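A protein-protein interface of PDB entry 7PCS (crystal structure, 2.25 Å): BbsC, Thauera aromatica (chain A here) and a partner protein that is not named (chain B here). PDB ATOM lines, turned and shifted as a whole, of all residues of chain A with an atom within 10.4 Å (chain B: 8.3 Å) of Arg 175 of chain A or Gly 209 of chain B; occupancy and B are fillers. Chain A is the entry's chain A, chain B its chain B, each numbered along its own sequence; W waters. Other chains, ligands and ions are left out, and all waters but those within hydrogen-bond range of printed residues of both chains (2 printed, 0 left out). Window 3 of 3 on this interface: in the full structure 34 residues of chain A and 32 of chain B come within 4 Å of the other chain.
OH of Tyr 230 of chain A lies within hydrogen-bond range of O of Leu 185 of chain B (2.8 Å).
The side-chain hydroxyl (OH) of Tyr 230 of chain A is in hydrogen-bond range of the side-chain amide oxygen (OE1) of Gln 206 of chain B (2.6 Å).
The backbone NH (N) of Gly 212 of chain B sits close to the side-chain hydroxyl (OH) of Tyr 230 of chain A (3.3 Å).
The backbone carbonyl oxygen (O) of Tyr 230 of chain A lies within hydrogen-bond range of the backbone NH (N) of Gly 241 of chain B.
NH1 of Arg 175 of chain A lies within hydrogen-bond range of O of Pro 207 of chain B (3.4 Å).
OH of Tyr 230 of chain A sits at hydrogen-bond distance from O of Cys 240 of chain B, at 3.2 Å.
The backbone NH (N) of Gly 212 of chain B sits at hydrogen-bond distance from the backbone carbonyl oxygen (O) of Leu 185 of chain B (3.3 Å).
The backbone carbonyl oxygen (O) of Cys 240 of chain B sits close to the side-chain amide oxygen (OE1) of Gln 206 of chain B (3.4 Å).
The backbone carbonyl oxygen (O) of Lys 210 of chain B lies within hydrogen-bond range of the side-chain hydroxyl (OG1) of Thr 208 of chain B.
OG1 of Thr 232 of chain A lies within hydrogen-bond range of N of Val 180 of chain A.
Pro 207 of chain B touches Leu 171 of chain A.
Ala 174 of chain A touches Pro 207 of chain B.
Ala 174 of chain A touches Thr 208 of chain B.
O of Gln 206 of chain B touches NH1 of Arg 175 of chain A (3.9 Å).
CA of Gly 209 of chain B touches NH2 of Arg 175 of chain A (3.9 Å).
Tyr 230 of chain A touches Thr 208 of chain B (CE1 to OG1, 3.9 Å).
Tyr 230 of chain A touches Lys 210 of chain B.
CE1 of Tyr 230 of chain A touches C of Leu 211 of chain B (3.9 Å).
Gly 241 of chain B touches Thr 232 of chain A (C to CG2, 3.8 Å).
Gly 134 of chain A touches none of the printed residues of chain B.
Of chain B, only Pro 207 (3.6 Å) and Thr 208 (3.9 Å) come within 4 Å of Ala 174 of chain A.
Of the printed residues of chain B, Arg 175 of chain A touches Gln 206 (3.9 Å), Pro 207 (3.4 Å) and Gly 209 (3.9 Å).
Of the printed residues of chain B, Thr 232 of chain A touches Gly 241 (3.8 Å).
Of the printed residues of chain A, Leu 185 of chain B touches Tyr 230.
Of the printed residues of chain A, Pro 207 of chain B touches Leu 171, Ala 174 and Arg 175.
Lys 210 of chain B touches just one residue of chain A: Tyr 230.
Printed residues of chain A within 4 Å of Leu 211 of chain B: Tyr 230.
Printed residues of chain A within 4 Å of Gly 212 of chain B: Tyr 230 (3.2 Å).
Of the printed residues of chain A, Cys 240 of chain B touches Tyr 230.
The nearest residue of chain A that does not touch Gly 209 of chain B is Ala 174 of chain A (5.9 Å).
Of the 25 printed residues of chain A, 5 touch a printed residue of chain B.
Printed residues of chain A that touch a printed residue of chain B: Leu 171, Ala 174, Arg 175, Tyr 230 and Thr 232.
Among the printed residues, no Asp or Glu carboxylate lies within 4 Å of a Lys or Arg side-chain nitrogen of the other chain.
Water W2 lies within hydrogen-bond range of NE2 of Gln 206 of chain B (2.7 Å), O of Cys 240 of chain B (2.7 Å), N of Leu 185 of chain B (3.1 Å) and OH of Tyr 230 of chain A (3.2 Å).
Water W1 lies within hydrogen-bond range of SG of Cys 240 of chain B, N of Thr 232 of chain A and O of Tyr 230 of chain A.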
ATOM      1  N   VAL A 127       8.307   3.938  19.416  1.00  0.00           N
ATOM      2  CA  VAL A 127       6.944   4.267  18.990  1.00  0.00           C
ATOM      3  C   VAL A 127       5.916   3.877  20.046  1.00  0.00           C
ATOM      4  O   VAL A 127       5.040   4.698  20.361  1.00  0.00           O
ATOM      5  CB  VAL A 127       6.651   3.640  17.625  1.00  0.00           C
ATOM      6  CG1 VAL A 127       5.160   3.707  17.325  1.00  0.00           C
ATOM      7  CG2 VAL A 127       7.455   4.330  16.533  1.00  0.00           C
ATOM      8  N   MET A 130       5.767   6.507  22.593  1.00  0.00           N
ATOM      9  CA  MET A 130       5.249   7.776  22.088  1.00  0.00           C
ATOM     10  C   MET A 130       3.729   7.757  21.980  1.00  0.00           C
ATOM     11  O   MET A 130       3.055   8.716  22.375  1.00  0.00           O
ATOM     12  CB  MET A 130       5.864   8.096  20.726  1.00  0.00           C
ATOM     13  CG  MET A 130       7.302   8.578  20.778  1.00  0.00           C
ATOM     14  SD  MET A 130       8.115   8.508  19.157  1.00  0.00           S
ATOM     15  CE  MET A 130       9.583   9.486  19.491  1.00  0.00           C
ATOM     16  N   ARG A 131       3.171   6.681  21.426  1.00  0.00           N
ATOM     17  CA  ARG A 131       1.719   6.576  21.319  1.00  0.00           C
ATOM     18  C   ARG A 131       1.065   6.574  22.697  1.00  0.00           C
ATOM     19  O   ARG A 131      -0.021   7.137  22.882  1.00  0.00           O
ATOM     20  CB  ARG A 131       1.351   5.307  20.552  1.00  0.00           C
ATOM     21  CG  ARG A 131       1.901   5.242  19.135  1.00  0.00           C
ATOM     22  CD  ARG A 131       1.399   3.992  18.421  1.00  0.00           C
ATOM     23  NE  ARG A 131      -0.059   3.935  18.377  1.00  0.00           N
ATOM     24  CZ  ARG A 131      -0.753   2.902  17.915  1.00  0.00           C
ATOM     25  NH1 ARG A 131      -0.151   1.827  17.432  1.00  0.00           N
ATOM     26  NH2 ARG A 131      -2.084   2.946  17.946  1.00  0.00           N
ATOM     27  N   GLU A 132       1.716   5.944  23.678  1.00  0.00           N
ATOM     28  CA  GLU A 132       1.174   5.911  25.034  1.00  0.00           C
ATOM     29  C   GLU A 132       1.172   7.301  25.658  1.00  0.00           C
ATOM     30  O   GLU A 132       0.195   7.698  26.307  1.00  0.00           O
ATOM     31  CB  GLU A 132       1.975   4.928  25.883  1.00  0.00           C
ATOM     32  CG  GLU A 132       1.568   4.857  27.330  1.00  0.00           C
ATOM     33  CD  GLU A 132       2.450   3.906  28.121  1.00  0.00           C
ATOM     34  OE1 GLU A 132       3.649   4.209  28.311  1.00  0.00           O
ATOM     35  OE2 GLU A 132       1.947   2.836  28.525  1.00  0.00           O
ATOM     36  N   ALA A 133       2.261   8.055  25.485  1.00  0.00           N
ATOM     37  CA  ALA A 133       2.318   9.417  26.001  1.00  0.00           C
ATOM     38  C   ALA A 133       1.499  10.393  25.171  1.00  0.00           C
ATOM     39  O   ALA A 133       1.276  11.526  25.612  1.00  0.00           O
ATOM     40  CB  ALA A 133       3.767   9.896  26.068  1.00  0.00           C
ATOM     41  N   GLY A 134       1.062   9.992  23.983  1.00  0.00           N
ATOM     42  CA  GLY A 134       0.253  10.852  23.148  1.00  0.00           C
ATOM     43  C   GLY A 134       1.016  11.892  22.363  1.00  0.00           C
ATOM     44  O   GLY A 134       0.390  12.753  21.733  1.00  0.00           O
ATOM     45  N   PHE A 135       2.344  11.842  22.377  1.00  0.00           N
ATOM     46  CA  PHE A 135       3.152  12.764  21.597  1.00  0.00           C
ATOM     47  C   PHE A 135       4.397  12.030  21.129  1.00  0.00           C
ATOM     48  O   PHE A 135       5.026  11.305  21.902  1.00  0.00           O
ATOM     49  CB  PHE A 135       3.555  14.009  22.398  1.00  0.00           C
ATOM     50  CG  PHE A 135       4.434  14.964  21.633  1.00  0.00           C
ATOM     51  CD1 PHE A 135       5.793  14.736  21.519  1.00  0.00           C
ATOM     52  CD2 PHE A 135       3.897  16.089  21.028  1.00  0.00           C
ATOM     53  CE1 PHE A 135       6.603  15.604  20.814  1.00  0.00           C
ATOM     54  CE2 PHE A 135       4.702  16.968  20.322  1.00  0.00           C
ATOM     55  CZ  PHE A 135       6.059  16.724  20.217  1.00  0.00           C
ATOM     56  N   GLY A 136       4.754  12.243  19.868  1.00  0.00           N
ATOM     57  CA  GLY A 136       5.960  11.665  19.316  1.00  0.00           C
ATOM     58  C   GLY A 136       6.333  12.302  17.996  1.00  0.00           C
ATOM     59  O   GLY A 136       5.458  12.651  17.199  1.00  0.00           O
ATOM     60  N   ARG A 137       7.631  12.465  17.763  1.00  0.00           N
ATOM     61  CA  ARG A 137       8.163  12.982  16.506  1.00  0.00           C
ATOM     62  C   ARG A 137       9.324  12.084  16.109  1.00  0.00           C
ATOM     63  O   ARG A 137      10.368  12.090  16.769  1.00  0.00           O
ATOM     64  CB  ARG A 137       8.621  14.434  16.648  1.00  0.00           C
ATOM     65  CG  ARG A 137       7.522  15.416  17.023  1.00  0.00           C
ATOM     66  CD  ARG A 137       6.623  15.774  15.836  1.00  0.00           C
ATOM     67  NE  ARG A 137       5.648  16.792  16.209  1.00  0.00           N
ATOM     68  CZ  ARG A 137       4.481  16.544  16.792  1.00  0.00           C
ATOM     69  NH1 ARG A 137       4.098  15.311  17.076  1.00  0.00           N
ATOM     70  NH2 ARG A 137       3.678  17.560  17.091  1.00  0.00           N
ATOM     71  N   ALA A 168       4.314   3.264   6.824  1.00  0.00           N
ATOM     72  CA  ALA A 168       3.467   2.283   7.501  1.00  0.00           C
ATOM     73  C   ALA A 168       3.220   2.682   8.952  1.00  0.00           C
ATOM     74  O   ALA A 168       2.074   2.715   9.417  1.00  0.00           O
ATOM     75  CB  ALA A 168       4.104   0.898   7.424  1.00  0.00           C
ATOM     76  N   LEU A 169       4.289   2.994   9.682  1.00  0.00           N
ATOM     77  CA  LEU A 169       4.150   3.362  11.085  1.00  0.00           C
ATOM     78  C   LEU A 169       3.556   4.756  11.255  1.00  0.00           C
ATOM     79  O   LEU A 169       2.904   5.028  12.268  1.00  0.00           O
ATOM     80  CB  LEU A 169       5.507   3.279  11.773  1.00  0.00           C
ATOM     81  CG  LEU A 169       6.126   1.883  11.836  1.00  0.00           C
ATOM     82  CD1 LEU A 169       7.438   1.910  12.575  1.00  0.00           C
ATOM     83  CD2 LEU A 169       5.148   0.914  12.503  1.00  0.00           C
ATOM     84  N   ALA A 170       3.775   5.655  10.295  1.00  0.00           N
ATOM     85  CA  ALA A 170       3.079   6.933  10.332  1.00  0.00           C
ATOM     86  C   ALA A 170       1.576   6.713  10.415  1.00  0.00           C
ATOM     87  O   ALA A 170       0.889   7.298  11.261  1.00  0.00           O
ATOM     88  CB  ALA A 170       3.430   7.759   9.096  1.00  0.00           C
ATOM     89  N   LEU A 171       1.050   5.859   9.537  1.00  0.00           N
ATOM     90  CA  LEU A 171      -0.380   5.576   9.545  1.00  0.00           C
ATOM     91  C   LEU A 171      -0.783   4.808  10.795  1.00  0.00           C
ATOM     92  O   LEU A 171      -1.843   5.073  11.372  1.00  0.00           O
ATOM     93  CB  LEU A 171      -0.759   4.789   8.292  1.00  0.00           C
ATOM     94  CG  LEU A 171      -0.791   5.571   6.982  1.00  0.00           C
ATOM     95  CD1 LEU A 171      -0.847   4.634   5.799  1.00  0.00           C
ATOM     96  CD2 LEU A 171      -2.001   6.507   6.992  1.00  0.00           C
ATOM     97  N   GLU A 172       0.055   3.870  11.243  1.00  0.00           N
ATOM     98  CA  GLU A 172      -0.315   3.040  12.384  1.00  0.00           C
ATOM     99  C   GLU A 172      -0.382   3.846  13.673  1.00  0.00           C
ATOM    100  O   GLU A 172      -1.166   3.517  14.571  1.00  0.00           O
ATOM    101  CB  GLU A 172       0.676   1.886  12.539  1.00  0.00           C
ATOM    102  CG  GLU A 172       0.167   0.754  13.397  1.00  0.00           C
ATOM    103  CD  GLU A 172       1.109  -0.441  13.421  1.00  0.00           C
ATOM    104  OE1 GLU A 172       1.596  -0.846  12.346  1.00  0.00           O
ATOM    105  OE2 GLU A 172       1.355  -0.980  14.516  1.00  0.00           O
ATOM    106  N   SER A 173       0.422   4.896  13.785  1.00  0.00           N
ATOM    107  CA  SER A 173       0.526   5.658  15.018  1.00  0.00           C
ATOM    108  C   SER A 173      -0.176   7.000  14.953  1.00  0.00           C
ATOM    109  O   SER A 173      -0.214   7.704  15.968  1.00  0.00           O
ATOM    110  CB  SER A 173       1.997   5.894  15.362  1.00  0.00           C
ATOM    111  OG  SER A 173       2.622   6.668  14.348  1.00  0.00           O
ATOM    112  N   ALA A 174      -0.732   7.371  13.795  1.00  0.00           N
ATOM    113  CA  ALA A 174      -1.208   8.737  13.599  1.00  0.00           C
ATOM    114  C   ALA A 174      -2.191   9.158  14.682  1.00  0.00           C
ATOM    115  O   ALA A 174      -2.132  10.286  15.179  1.00  0.00           O
ATOM    116  CB  ALA A 174      -1.851   8.873  12.217  1.00  0.00           C
ATOM    117  N   ARG A 175      -3.097   8.269  15.074  1.00  0.00           N
ATOM    118  CA  ARG A 175      -4.173   8.688  15.964  1.00  0.00           C
ATOM    119  C   ARG A 175      -3.666   9.113  17.337  1.00  0.00           C
ATOM    120  O   ARG A 175      -4.385   9.815  18.056  1.00  0.00           O
ATOM    121  CB  ARG A 175      -5.191   7.560  16.139  1.00  0.00           C
ATOM    122  CG  ARG A 175      -6.619   8.028  16.438  1.00  0.00           C
ATOM    123  CD  ARG A 175      -7.631   6.938  16.054  1.00  0.00           C
ATOM    124  NE  ARG A 175      -8.822   7.452  15.385  1.00  0.00           N
ATOM    125  CZ  ARG A 175      -9.010   7.402  14.074  1.00  0.00           C
ATOM    126  NH1 ARG A 175      -8.105   6.869  13.269  1.00  0.00           N
ATOM    127  NH2 ARG A 175     -10.127   7.904  13.556  1.00  0.00           N
ATOM    128  N   ASP A 176      -2.454   8.713  17.719  1.00  0.00           N
ATOM    129  CA  ASP A 176      -1.931   8.944  19.062  1.00  0.00           C
ATOM    130  C   ASP A 176      -0.859  10.032  19.094  1.00  0.00           C
ATOM    131  O   ASP A 176       0.110   9.949  19.850  1.00  0.00           O
ATOM    132  CB  ASP A 176      -1.376   7.651  19.648  1.00  0.00           C
ATOM    133  CG  ASP A 176      -2.427   6.567  19.757  1.00  0.00           C
ATOM    134  OD1 ASP A 176      -3.606   6.900  20.011  1.00  0.00           O
ATOM    135  OD2 ASP A 176      -2.076   5.378  19.593  1.00  0.00           O
ATOM    136  N   GLY A 177      -1.017  11.060  18.265  1.00  0.00           N
ATOM    137  CA  GLY A 177      -0.166  12.228  18.366  1.00  0.00           C
ATOM    138  C   GLY A 177       1.266  12.014  17.948  1.00  0.00           C
ATOM    139  O   GLY A 177       2.131  12.823  18.295  1.00  0.00           O
ATOM    140  N   VAL A 178       1.547  10.947  17.215  1.00  0.00           N
ATOM    141  CA  VAL A 178       2.893  10.637  16.760  1.00  0.00           C
ATOM    142  C   VAL A 178       2.975  10.896  15.261  1.00  0.00           C
ATOM    143  O   VAL A 178       2.027  10.613  14.518  1.00  0.00           O
ATOM    144  CB  VAL A 178       3.271   9.179  17.087  1.00  0.00           C
ATOM    145  CG1 VAL A 178       4.715   8.909  16.712  1.00  0.00           C
ATOM    146  CG2 VAL A 178       3.028   8.885  18.545  1.00  0.00           C
ATOM    147  N   THR A 179       4.102  11.452  14.822  1.00  0.00           N
ATOM    148  CA  THR A 179       4.399  11.629  13.406  1.00  0.00           C
ATOM    149  C   THR A 179       5.715  10.931  13.087  1.00  0.00           C
ATOM    150  O   THR A 179       6.635  10.917  13.910  1.00  0.00           O
ATOM    151  CB  THR A 179       4.490  13.111  13.008  1.00  0.00           C
ATOM    152  OG1 THR A 179       5.721  13.664  13.488  1.00  0.00           O
ATOM    153  CG2 THR A 179       3.321  13.888  13.575  1.00  0.00           C
ATOM    154  N   VAL A 180       5.798  10.355  11.891  1.00  0.00           N
ATOM    155  CA  VAL A 180       7.001   9.684  11.414  1.00  0.00           C
ATOM    156  C   VAL A 180       7.310  10.240  10.034  1.00  0.00           C
ATOM    157  O   VAL A 180       6.519  10.059   9.102  1.00  0.00           O
ATOM    158  CB  VAL A 180       6.831   8.157  11.354  1.00  0.00           C
ATOM    159  CG1 VAL A 180       8.163   7.494  11.053  1.00  0.00           C
ATOM    160  CG2 VAL A 180       6.243   7.631  12.657  1.00  0.00           C
ATOM    161  N   LYS A 229       2.430  18.970  13.860  1.00  0.00           N
ATOM    162  CA  LYS A 229       1.584  17.860  14.290  1.00  0.00           C
ATOM    163  C   LYS A 229       0.687  17.329  13.178  1.00  0.00           C
ATOM    164  O   LYS A 229       0.063  16.281  13.369  1.00  0.00           O
ATOM    165  CB  LYS A 229       0.727  18.261  15.503  1.00  0.00           C
ATOM    166  CG  LYS A 229       0.196  19.683  15.495  1.00  0.00           C
ATOM    167  CD  LYS A 229      -1.235  19.770  14.962  1.00  0.00           C
ATOM    168  CE  LYS A 229      -1.800  21.186  15.154  1.00  0.00           C
ATOM    169  NZ  LYS A 229      -3.119  21.375  14.474  1.00  0.00           N
ATOM    170  N   TYR A 230       0.596  18.021  12.042  1.00  0.00           N
ATOM    171  CA  TYR A 230      -0.229  17.590  10.919  1.00  0.00           C
ATOM    172  C   TYR A 230       0.612  17.175   9.715  1.00  0.00           C
ATOM    173  O   TYR A 230       0.070  16.999   8.619  1.00  0.00           O
ATOM    174  CB  TYR A 230      -1.201  18.705  10.523  1.00  0.00           C
ATOM    175  CG  TYR A 230      -2.471  18.215   9.855  1.00  0.00           C
ATOM    176  CD1 TYR A 230      -3.362  17.382  10.526  1.00  0.00           C
ATOM    177  CD2 TYR A 230      -2.787  18.600   8.558  1.00  0.00           C
ATOM    178  CE1 TYR A 230      -4.522  16.939   9.915  1.00  0.00           C
ATOM    179  CE2 TYR A 230      -3.943  18.165   7.941  1.00  0.00           C
ATOM    180  CZ  TYR A 230      -4.806  17.336   8.622  1.00  0.00           C
ATOM    181  OH  TYR A 230      -5.957  16.901   8.007  1.00  0.00           O
ATOM    182  N   THR A 232       3.014  14.208   8.474  1.00  0.00           N
ATOM    183  CA  THR A 232       3.486  12.869   8.771  1.00  0.00           C
ATOM    184  C   THR A 232       3.548  12.062   7.483  1.00  0.00           C
ATOM    185  O   THR A 232       2.837  12.345   6.514  1.00  0.00           O
ATOM    186  CB  THR A 232       2.592  12.165   9.800  1.00  0.00           C
ATOM    187  OG1 THR A 232       3.326  11.097  10.413  1.00  0.00           O
ATOM    188  CG2 THR A 232       1.344  11.600   9.132  1.00  0.00           C
ATOM    189  N   LEU B 185      -6.890  17.993   4.277  1.00  0.00           N
ATOM    190  CA  LEU B 185      -8.154  18.542   4.751  1.00  0.00           C
ATOM    191  C   LEU B 185      -7.901  19.512   5.898  1.00  0.00           C
ATOM    192  O   LEU B 185      -7.229  19.163   6.871  1.00  0.00           O
ATOM    193  CB  LEU B 185      -9.055  17.392   5.181  1.00  0.00           C
ATOM    194  CG  LEU B 185     -10.424  17.627   5.787  1.00  0.00           C
ATOM    195  CD1 LEU B 185     -11.442  18.062   4.807  1.00  0.00           C
ATOM    196  CD2 LEU B 185     -10.835  16.234   6.397  1.00  0.00           C
ATOM    197  N   LEU B 202     -15.796  12.727   6.582  1.00  0.00           N
ATOM    198  CA  LEU B 202     -14.433  13.107   6.226  1.00  0.00           C
ATOM    199  C   LEU B 202     -13.475  12.865   7.386  1.00  0.00           C
ATOM    200  O   LEU B 202     -12.417  12.244   7.213  1.00  0.00           O
ATOM    201  CB  LEU B 202     -14.402  14.566   5.786  1.00  0.00           C
ATOM    202  CG  LEU B 202     -15.283  14.840   4.566  1.00  0.00           C
ATOM    203  CD1 LEU B 202     -16.790  14.868   4.997  1.00  0.00           C
ATOM    204  CD2 LEU B 202     -14.979  16.073   3.777  1.00  0.00           C
ATOM    205  N   LEU B 203     -13.824  13.359   8.577  1.00  0.00           N
ATOM    206  CA  LEU B 203     -13.018  13.085   9.763  1.00  0.00           C
ATOM    207  C   LEU B 203     -12.675  11.604   9.866  1.00  0.00           C
ATOM    208  O   LEU B 203     -11.538  11.242  10.193  1.00  0.00           O
ATOM    209  CB  LEU B 203     -13.769  13.543  11.017  1.00  0.00           C
ATOM    210  CG  LEU B 203     -13.621  14.999  11.454  1.00  0.00           C
ATOM    211  CD1 LEU B 203     -14.485  15.305  12.653  1.00  0.00           C
ATOM    212  CD2 LEU B 203     -12.164  15.284  11.792  1.00  0.00           C
ATOM    213  N   SER B 204     -13.650  10.731   9.603  1.00  0.00           N
ATOM    214  CA  SER B 204     -13.413   9.294   9.660  1.00  0.00           C
ATOM    215  C   SER B 204     -12.337   8.843   8.680  1.00  0.00           C
ATOM    216  O   SER B 204     -11.734   7.782   8.883  1.00  0.00           O
ATOM    217  CB  SER B 204     -14.716   8.541   9.385  1.00  0.00           C
ATOM    218  OG  SER B 204     -15.214   8.851   8.094  1.00  0.00           O
ATOM    219  N   ARG B 205     -12.086   9.616   7.625  1.00  0.00           N
ATOM    220  CA  ARG B 205     -11.039   9.326   6.652  1.00  0.00           C
ATOM    221  C   ARG B 205      -9.684   9.915   7.044  1.00  0.00           C
ATOM    222  O   ARG B 205      -8.733   9.828   6.260  1.00  0.00           O
ATOM    223  CB  ARG B 205     -11.449   9.877   5.282  1.00  0.00           C
ATOM    224  CG  ARG B 205     -12.797   9.411   4.748  1.00  0.00           C
ATOM    225  CD  ARG B 205     -12.967   7.899   4.581  1.00  0.00           C
ATOM    226  NE  ARG B 205     -13.022   7.564   3.159  1.00  0.00           N
ATOM    227  CZ  ARG B 205     -13.014   6.335   2.658  1.00  0.00           C
ATOM    228  NH1 ARG B 205     -12.874   5.274   3.433  1.00  0.00           N
ATOM    229  NH2 ARG B 205     -13.155   6.169   1.344  1.00  0.00           N
ATOM    230  N   GLN B 206      -9.571  10.503   8.234  1.00  0.00           N
ATOM    231  CA  GLN B 206      -8.328  11.125   8.666  1.00  0.00           C
ATOM    232  C   GLN B 206      -7.527  10.187   9.552  1.00  0.00           C
ATOM    233  O   GLN B 206      -8.057   9.707  10.570  1.00  0.00           O
ATOM    234  CB  GLN B 206      -8.623  12.419   9.414  1.00  0.00           C
ATOM    235  CG  GLN B 206      -9.138  13.538   8.550  1.00  0.00           C
ATOM    236  CD  GLN B 206      -8.092  14.029   7.586  1.00  0.00           C
ATOM    237  OE1 GLN B 206      -7.060  14.553   7.994  1.00  0.00           O
ATOM    238  NE2 GLN B 206      -8.344  13.849   6.299  1.00  0.00           N
ATOM    239  N   PRO B 207      -6.264   9.892   9.218  1.00  0.00           N
ATOM    240  CA  PRO B 207      -5.467   9.041  10.120  1.00  0.00           C
ATOM    241  C   PRO B 207      -5.353   9.601  11.528  1.00  0.00           C
ATOM    242  O   PRO B 207      -5.445   8.843  12.502  1.00  0.00           O
ATOM    243  CB  PRO B 207      -4.099   8.976   9.425  1.00  0.00           C
ATOM    244  CG  PRO B 207      -4.427   9.169   7.953  1.00  0.00           C
ATOM    245  CD  PRO B 207      -5.553  10.184   7.955  1.00  0.00           C
ATOM    246  N   THR B 208      -5.140  10.912  11.666  1.00  0.00           N
ATOM    247  CA  THR B 208      -5.067  11.508  12.993  1.00  0.00           C
ATOM    248  C   THR B 208      -6.424  11.578  13.675  1.00  0.00           C
ATOM    249  O   THR B 208      -6.480  11.822  14.885  1.00  0.00           O
ATOM    250  CB  THR B 208      -4.484  12.922  12.917  1.00  0.00           C
ATOM    251  OG1 THR B 208      -5.312  13.741  12.084  1.00  0.00           O
ATOM    252  CG2 THR B 208      -3.078  12.899  12.344  1.00  0.00           C
ATOM    253  N   GLY B 209      -7.510  11.373  12.935  1.00  0.00           N
ATOM    254  CA  GLY B 209      -8.841  11.551  13.470  1.00  0.00           C
ATOM    255  C   GLY B 209      -9.237  12.987  13.718  1.00  0.00           C
ATOM    256  O   GLY B 209     -10.360  13.231  14.176  1.00  0.00           O
ATOM    257  N   LYS B 210      -8.363  13.945  13.423  1.00  0.00           N
ATOM    258  CA  LYS B 210      -8.621  15.354  13.659  1.00  0.00           C
ATOM    259  C   LYS B 210      -8.406  16.115  12.359  1.00  0.00           C
ATOM    260  O   LYS B 210      -7.774  15.623  11.420  1.00  0.00           O
ATOM    261  CB  LYS B 210      -7.713  15.915  14.766  1.00  0.00           C
ATOM    262  N   LEU B 211      -8.946  17.323  12.310  1.00  0.00           N
ATOM    263  CA  LEU B 211      -8.767  18.189  11.160  1.00  0.00           C
ATOM    264  C   LEU B 211      -7.487  19.000  11.309  1.00  0.00           C
ATOM    265  O   LEU B 211      -7.106  19.396  12.414  1.00  0.00           O
ATOM    266  CB  LEU B 211      -9.958  19.131  11.010  1.00  0.00           C
ATOM    267  CG  LEU B 211     -11.260  18.494  10.528  1.00  0.00           C
ATOM    268  CD1 LEU B 211     -12.364  19.565  10.693  1.00  0.00           C
ATOM    269  CD2 LEU B 211     -11.210  17.990   9.111  1.00  0.00           C
ATOM    270  N   GLY B 212      -6.832  19.258  10.179  1.00  0.00           N
ATOM    271  CA  GLY B 212      -5.763  20.235  10.165  1.00  0.00           C
ATOM    272  C   GLY B 212      -6.309  21.646  10.269  1.00  0.00           C
ATOM    273  O   GLY B 212      -7.444  21.928   9.893  1.00  0.00           O
ATOM    274  N   CYS B 240      -1.239  17.040   5.584  1.00  0.00           N
ATOM    275  CA  CYS B 240      -2.464  16.264   5.464  1.00  0.00           C
ATOM    276  C   CYS B 240      -2.803  15.420   6.682  1.00  0.00           C
ATOM    277  O   CYS B 240      -3.890  14.826   6.710  1.00  0.00           O
ATOM    278  CB  CYS B 240      -2.371  15.325   4.253  1.00  0.00           C
ATOM    279  SG  CYS B 240      -0.996  14.129   4.403  1.00  0.00           S
ATOM    280  N   GLY B 241      -1.924  15.329   7.674  1.00  0.00           N
ATOM    281  CA  GLY B 241      -2.185  14.426   8.774  1.00  0.00           C
ATOM    282  C   GLY B 241      -2.150  12.972   8.376  1.00  0.00           C
ATOM    283  O   GLY B 241      -2.776  12.139   9.037  1.00  0.00           O
HETATM  284  O   HOH W   1       1.421  15.295   5.966  1.00  0.00           O
HETATM  285  O   HOH W   2      -6.189  15.143   5.312  1.00  0.00           O
